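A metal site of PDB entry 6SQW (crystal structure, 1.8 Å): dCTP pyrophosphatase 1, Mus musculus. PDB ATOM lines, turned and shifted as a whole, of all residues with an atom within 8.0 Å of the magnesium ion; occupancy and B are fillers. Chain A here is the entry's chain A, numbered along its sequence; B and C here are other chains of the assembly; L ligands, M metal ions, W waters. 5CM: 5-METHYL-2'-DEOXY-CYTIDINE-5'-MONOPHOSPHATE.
O3' of the ligand lies within hydrogen-bond range of ND2 of Asn 125 of chain B, at 2.8 Å. O3' of the ligand is in hydrogen-bond range of OD1 of Asp 98 (2.7 Å). OP2 of the ligand lies within salt-bridge range of NH1 of Arg 128 of chain B (2.9 Å).
OE1 of Glu 63 is bound to the magnesium ion (2.0 Å). The magnesium ion is bound by the side-chain carboxylate (OE2) of Glu 66. OE1 of Glu 95 binds the magnesium ion (2.1 Å). Water W1 is bound to the magnesium ion (2.1 Å). The magnesium ion is bound by water W2 (2.1 Å). OD2 of Asp 98 is bound to the magnesium ion (2.1 Å). The magnesium ion has six donor atoms within binding distance.
Water W2 lies within hydrogen-bond range of the side-chain carboxylate of Glu 63 and an oxygen (OP3) of the ligand.
OD1 of Asp 98 lies within salt-bridge range of NZ of Lys 121 of chain B.
Within 4 Å of the magnesium ion: Glu 63, Glu 66, Glu 95 and Asp 98. The nearest printed residue that does not touch the magnesium ion is Lys 121 of chain B (4.9 Å).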
ATOM      1  N   ALA A  59      11.077 -25.283  -0.362  1.00  0.00           N
ATOM      2  CA  ALA A  59      11.930 -24.421   0.459  1.00  0.00           C
ATOM      3  C   ALA A  59      11.592 -22.947   0.119  1.00  0.00           C
ATOM      4  O   ALA A  59      11.478 -22.121   1.015  1.00  0.00           O
ATOM      5  CB  ALA A  59      13.375 -24.716   0.226  1.00  0.00           C
ATOM      6  N   GLY A  62       8.493 -21.937   1.849  1.00  0.00           N
ATOM      7  CA  GLY A  62       8.843 -21.659   3.224  1.00  0.00           C
ATOM      8  C   GLY A  62       9.421 -20.273   3.444  1.00  0.00           C
ATOM      9  O   GLY A  62       9.127 -19.584   4.420  1.00  0.00           O
ATOM     10  N   GLU A  63      10.278 -19.871   2.551  1.00  0.00           N
ATOM     11  CA  GLU A  63      10.880 -18.553   2.662  1.00  0.00           C
ATOM     12  C   GLU A  63       9.907 -17.407   2.373  1.00  0.00           C
ATOM     13  O   GLU A  63       9.945 -16.370   3.022  1.00  0.00           O
ATOM     14  CB  GLU A  63      12.092 -18.432   1.734  1.00  0.00           C
ATOM     15  CG  GLU A  63      13.144 -19.487   1.991  1.00  0.00           C
ATOM     16  CD  GLU A  63      13.740 -19.503   3.344  1.00  0.00           C
ATOM     17  OE1 GLU A  63      13.599 -18.486   4.094  1.00  0.00           O
ATOM     18  OE2 GLU A  63      14.422 -20.540   3.679  1.00  0.00           O
ATOM     19  N   VAL A  64       9.025 -17.617   1.424  1.00  0.00           N
ATOM     20  CA  VAL A  64       7.952 -16.649   1.181  1.00  0.00           C
ATOM     21  C   VAL A  64       7.116 -16.540   2.417  1.00  0.00           C
ATOM     22  O   VAL A  64       6.655 -15.452   2.752  1.00  0.00           O
ATOM     23  CB  VAL A  64       7.116 -17.056  -0.023  1.00  0.00           C
ATOM     24  CG1 VAL A  64       5.881 -16.188  -0.171  1.00  0.00           C
ATOM     25  CG2 VAL A  64       7.971 -16.951  -1.262  1.00  0.00           C
ATOM     26  N   GLY A  65       6.936 -17.640   3.141  1.00  0.00           N
ATOM     27  CA  GLY A  65       6.213 -17.602   4.406  1.00  0.00           C
ATOM     28  C   GLY A  65       6.902 -16.741   5.433  1.00  0.00           C
ATOM     29  O   GLY A  65       6.258 -15.931   6.075  1.00  0.00           O
ATOM     30  N   GLU A  66       8.219 -16.902   5.567  1.00  0.00           N
ATOM     31  CA  GLU A  66       8.967 -16.101   6.507  1.00  0.00           C
ATOM     32  C   GLU A  66       8.914 -14.613   6.151  1.00  0.00           C
ATOM     33  O   GLU A  66       8.819 -13.766   7.036  1.00  0.00           O
ATOM     34  CB  GLU A  66      10.418 -16.560   6.592  1.00  0.00           C
ATOM     35  CG  GLU A  66      10.524 -17.842   7.364  1.00  0.00           C
ATOM     36  CD  GLU A  66      11.964 -18.323   7.611  1.00  0.00           C
ATOM     37  OE1 GLU A  66      12.167 -18.712   8.752  1.00  0.00           O
ATOM     38  OE2 GLU A  66      12.849 -18.326   6.733  1.00  0.00           O
ATOM     39  N   LEU A  67       8.929 -14.330   4.852  1.00  0.00           N
ATOM     40  CA  LEU A  67       8.856 -12.938   4.381  1.00  0.00           C
ATOM     41  C   LEU A  67       7.461 -12.342   4.738  1.00  0.00           C
ATOM     42  O   LEU A  67       7.345 -11.262   5.309  1.00  0.00           O
ATOM     43  CB  LEU A  67       9.067 -12.922   2.875  1.00  0.00           C
ATOM     44  CG  LEU A  67       9.024 -11.588   2.130  1.00  0.00           C
ATOM     45  CD1 LEU A  67      10.168 -10.736   2.602  1.00  0.00           C
ATOM     46  CD2 LEU A  67       9.197 -11.840   0.638  1.00  0.00           C
ATOM     47  N   ALA A  91      16.037  -8.779   9.153  1.00  0.00           N
ATOM     48  CA  ALA A  91      15.145  -9.896   8.816  1.00  0.00           C
ATOM     49  C   ALA A  91      14.624  -9.769   7.425  1.00  0.00           C
ATOM     50  O   ALA A  91      14.584 -10.762   6.703  1.00  0.00           O
ATOM     51  CB  ALA A  91      13.997  -9.951   9.820  1.00  0.00           C
ATOM     52  N   GLU A  94      17.253 -10.603   4.923  1.00  0.00           N
ATOM     53  CA  GLU A  94      17.562 -12.002   4.969  1.00  0.00           C
ATOM     54  C   GLU A  94      16.509 -12.850   4.243  1.00  0.00           C
ATOM     55  O   GLU A  94      16.870 -13.745   3.471  1.00  0.00           O
ATOM     56  CB  GLU A  94      17.691 -12.508   6.423  1.00  0.00           C
ATOM     57  CG  GLU A  94      18.972 -12.055   7.116  1.00  0.00           C
ATOM     58  CD  GLU A  94      18.826 -12.048   8.633  1.00  0.00           C
ATOM     59  OE1 GLU A  94      17.942 -12.753   9.163  1.00  0.00           O
ATOM     60  OE2 GLU A  94      19.598 -11.325   9.335  1.00  0.00           O
ATOM     61  N   GLU A  95      15.236 -12.562   4.461  1.00  0.00           N
ATOM     62  CA  GLU A  95      14.177 -13.354   3.834  1.00  0.00           C
ATOM     63  C   GLU A  95      14.021 -13.044   2.385  1.00  0.00           C
ATOM     64  O   GLU A  95      13.807 -13.952   1.604  1.00  0.00           O
ATOM     65  CB  GLU A  95      12.848 -13.204   4.575  1.00  0.00           C
ATOM     66  CG  GLU A  95      12.886 -13.585   6.051  1.00  0.00           C
ATOM     67  CD  GLU A  95      13.615 -14.877   6.393  1.00  0.00           C
ATOM     68  OE1 GLU A  95      13.726 -15.838   5.577  1.00  0.00           O
ATOM     69  OE2 GLU A  95      14.089 -14.994   7.511  1.00  0.00           O
ATOM     70  N   LEU A  96      14.154 -11.782   1.991  1.00  0.00           N
ATOM     71  CA  LEU A  96      14.150 -11.477   0.587  1.00  0.00           C
ATOM     72  C   LEU A  96      15.270 -12.267  -0.120  1.00  0.00           C
ATOM     73  O   LEU A  96      15.098 -12.772  -1.239  1.00  0.00           O
ATOM     74  CB  LEU A  96      14.322  -9.991   0.357  1.00  0.00           C
ATOM     75  CG  LEU A  96      13.178  -9.059   0.650  1.00  0.00           C
ATOM     76  CD1 LEU A  96      13.659  -7.607   0.727  1.00  0.00           C
ATOM     77  CD2 LEU A  96      12.076  -9.213  -0.356  1.00  0.00           C
ATOM     78  N   SER A  97      16.424 -12.360   0.557  1.00  0.00           N
ATOM     79  CA  SER A  97      17.593 -13.065   0.023  1.00  0.00           C
ATOM     80  C   SER A  97      17.330 -14.573  -0.061  1.00  0.00           C
ATOM     81  O   SER A  97      17.650 -15.182  -1.063  1.00  0.00           O
ATOM     82  CB  SER A  97      18.836 -12.786   0.873  1.00  0.00           C
ATOM     83  OG  SER A  97      19.169 -11.396   0.856  1.00  0.00           O
ATOM     84  N   ASP A  98      16.787 -15.169   1.011  1.00  0.00           N
ATOM     85  CA  ASP A  98      16.424 -16.596   0.989  1.00  0.00           C
ATOM     86  C   ASP A  98      15.482 -16.902  -0.159  1.00  0.00           C
ATOM     87  O   ASP A  98      15.680 -17.919  -0.843  1.00  0.00           O
ATOM     88  CB  ASP A  98      15.801 -17.069   2.289  1.00  0.00           C
ATOM     89  CG  ASP A  98      16.759 -17.211   3.427  1.00  0.00           C
ATOM     90  OD1 ASP A  98      17.977 -17.375   3.187  1.00  0.00           O
ATOM     91  OD2 ASP A  98      16.248 -17.168   4.572  1.00  0.00           O
ATOM     92  N   VAL A  99      14.484 -16.056  -0.407  1.00  0.00           N
ATOM     93  CA  VAL A  99      13.618 -16.283  -1.527  1.00  0.00           C
ATOM     94  C   VAL A  99      14.424 -16.293  -2.839  1.00  0.00           C
ATOM     95  O   VAL A  99      14.260 -17.192  -3.681  1.00  0.00           O
ATOM     96  CB  VAL A  99      12.484 -15.260  -1.600  1.00  0.00           C
ATOM     97  CG1 VAL A  99      11.658 -15.482  -2.848  1.00  0.00           C
ATOM     98  CG2 VAL A  99      11.573 -15.404  -0.385  1.00  0.00           C
ATOM     99  N   TYR A 102      16.760 -19.511  -3.333  1.00  0.00           N
ATOM    100  CA  TYR A 102      16.058 -20.686  -3.790  1.00  0.00           C
ATOM    101  C   TYR A 102      15.515 -20.504  -5.171  1.00  0.00           C
ATOM    102  O   TYR A 102      15.440 -21.461  -5.923  1.00  0.00           O
ATOM    103  CB  TYR A 102      14.989 -21.131  -2.809  1.00  0.00           C
ATOM    104  CG  TYR A 102      15.554 -21.776  -1.579  1.00  0.00           C
ATOM    105  CD1 TYR A 102      16.371 -22.893  -1.658  1.00  0.00           C
ATOM    106  CD2 TYR A 102      15.177 -21.344  -0.319  1.00  0.00           C
ATOM    107  CE1 TYR A 102      16.836 -23.520  -0.509  1.00  0.00           C
ATOM    108  CE2 TYR A 102      15.622 -21.965   0.816  1.00  0.00           C
ATOM    109  CZ  TYR A 102      16.444 -23.043   0.716  1.00  0.00           C
ATOM    110  OH  TYR A 102      16.874 -23.627   1.858  1.00  0.00           O
ATOM    111  N   LYS B 121      23.589 -12.872   3.254  1.00  0.00           N
ATOM    112  CA  LYS B 121      22.849 -14.082   3.638  1.00  0.00           C
ATOM    113  C   LYS B 121      23.666 -15.350   3.370  1.00  0.00           C
ATOM    114  O   LYS B 121      23.692 -16.231   4.221  1.00  0.00           O
ATOM    115  CB  LYS B 121      21.473 -14.163   2.969  1.00  0.00           C
ATOM    116  CG  LYS B 121      20.565 -15.257   3.558  1.00  0.00           C
ATOM    117  CD  LYS B 121      20.456 -15.126   5.075  1.00  0.00           C
ATOM    118  CE  LYS B 121      19.314 -15.903   5.695  1.00  0.00           C
ATOM    119  NZ  LYS B 121      19.407 -17.373   5.491  1.00  0.00           N
ATOM    120  N   ASN B 125      24.707 -18.088   5.899  1.00  0.00           N
ATOM    121  CA  ASN B 125      24.451 -19.513   5.606  1.00  0.00           C
ATOM    122  C   ASN B 125      25.703 -20.391   5.850  1.00  0.00           C
ATOM    123  O   ASN B 125      25.623 -21.468   6.476  1.00  0.00           O
ATOM    124  CB  ASN B 125      23.983 -19.703   4.163  1.00  0.00           C
ATOM    125  CG  ASN B 125      22.594 -19.136   3.909  1.00  0.00           C
ATOM    126  OD1 ASN B 125      21.857 -18.838   4.848  1.00  0.00           O
ATOM    127  ND2 ASN B 125      22.242 -18.965   2.632  1.00  0.00           N
ATOM    128  N   ARG B 128      26.111 -20.766   9.642  1.00  0.00           N
ATOM    129  CA  ARG B 128      25.128 -21.641  10.241  1.00  0.00           C
ATOM    130  C   ARG B 128      25.371 -23.098   9.863  1.00  0.00           C
ATOM    131  O   ARG B 128      25.050 -23.964  10.617  1.00  0.00           O
ATOM    132  CB  ARG B 128      23.682 -21.184   9.934  1.00  0.00           C
ATOM    133  CG  ARG B 128      23.334 -19.872  10.651  1.00  0.00           C
ATOM    134  CD  ARG B 128      21.996 -19.171  10.307  1.00  0.00           C
ATOM    135  NE  ARG B 128      21.692 -19.360   8.902  1.00  0.00           N
ATOM    136  CZ  ARG B 128      20.893 -20.317   8.418  1.00  0.00           C
ATOM    137  NH1 ARG B 128      20.253 -21.176   9.238  1.00  0.00           N
ATOM    138  NH2 ARG B 128      20.741 -20.413   7.063  1.00  0.00           N
ATOM    139  N   GLU C  69       7.883 -26.134   5.291  1.00  0.00           N
ATOM    140  CA  GLU C  69       9.175 -26.392   5.913  1.00  0.00           C
ATOM    141  C   GLU C  69       9.302 -27.838   6.371  1.00  0.00           C
ATOM    142  O   GLU C  69      10.391 -28.438   6.292  1.00  0.00           O
ATOM    143  CB  GLU C  69       9.444 -25.470   7.093  1.00  0.00           C
ATOM    144  CG  GLU C  69       9.856 -24.034   6.746  1.00  0.00           C
ATOM    145  CD  GLU C  69       9.971 -23.094   7.980  1.00  0.00           C
ATOM    146  OE1 GLU C  69       9.763 -23.588   9.136  1.00  0.00           O
ATOM    147  OE2 GLU C  69      10.233 -21.845   7.814  1.00  0.00           O
HETATM  148  N1  5CM L   1      20.339 -23.655   2.323  1.00  0.00           N
HETATM  149  C2  5CM L   1      20.404 -24.456   1.178  1.00  0.00           C
HETATM  150  N3  5CM L   1      20.149 -25.791   1.238  1.00  0.00           N
HETATM  151  C4  5CM L   1      19.913 -26.400   2.431  1.00  0.00           C
HETATM  152  C5  5CM L   1      19.837 -25.574   3.654  1.00  0.00           C
HETATM  153  C5A 5CM L   1      19.543 -26.164   5.040  1.00  0.00           C
HETATM  154  C6  5CM L   1      20.094 -24.215   3.527  1.00  0.00           C
HETATM  155  O2  5CM L   1      20.648 -23.893   0.081  1.00  0.00           O
HETATM  156  N4  5CM L   1      19.664 -27.728   2.463  1.00  0.00           N
HETATM  157  C1' 5CM L   1      20.603 -22.205   2.189  1.00  0.00           C
HETATM  158  C2' 5CM L   1      19.629 -21.458   1.274  1.00  0.00           C
HETATM  159  C3' 5CM L   1      18.997 -20.323   2.133  1.00  0.00           C
HETATM  160  C4' 5CM L   1      19.384 -20.696   3.575  1.00  0.00           C
HETATM  161  O4' 5CM L   1      20.533 -21.576   3.488  1.00  0.00           O
HETATM  162  O3' 5CM L   1      19.542 -19.020   1.781  1.00  0.00           O
HETATM  163  C5' 5CM L   1      18.280 -21.411   4.359  1.00  0.00           C
HETATM  164  O5' 5CM L   1      18.742 -21.882   5.665  1.00  0.00           O
HETATM  165  P   5CM L   1      17.676 -22.233   6.852  1.00  0.00           P
HETATM  166  OP1 5CM L   1      16.588 -23.119   6.204  1.00  0.00           O
HETATM  167  OP2 5CM L   1      18.501 -23.002   7.876  1.00  0.00           O
HETATM  168  OP3 5CM L   1      17.243 -20.888   7.389  1.00  0.00           O
HETATM  169 MG    MG M   1      14.552 -17.742   5.723  1.00  0.00          MG
HETATM  170  O   HOH W   1      15.467 -17.385   7.558  1.00  0.00           O
HETATM  171  O   HOH W   2      15.242 -19.721   6.062  1.00  0.00           O
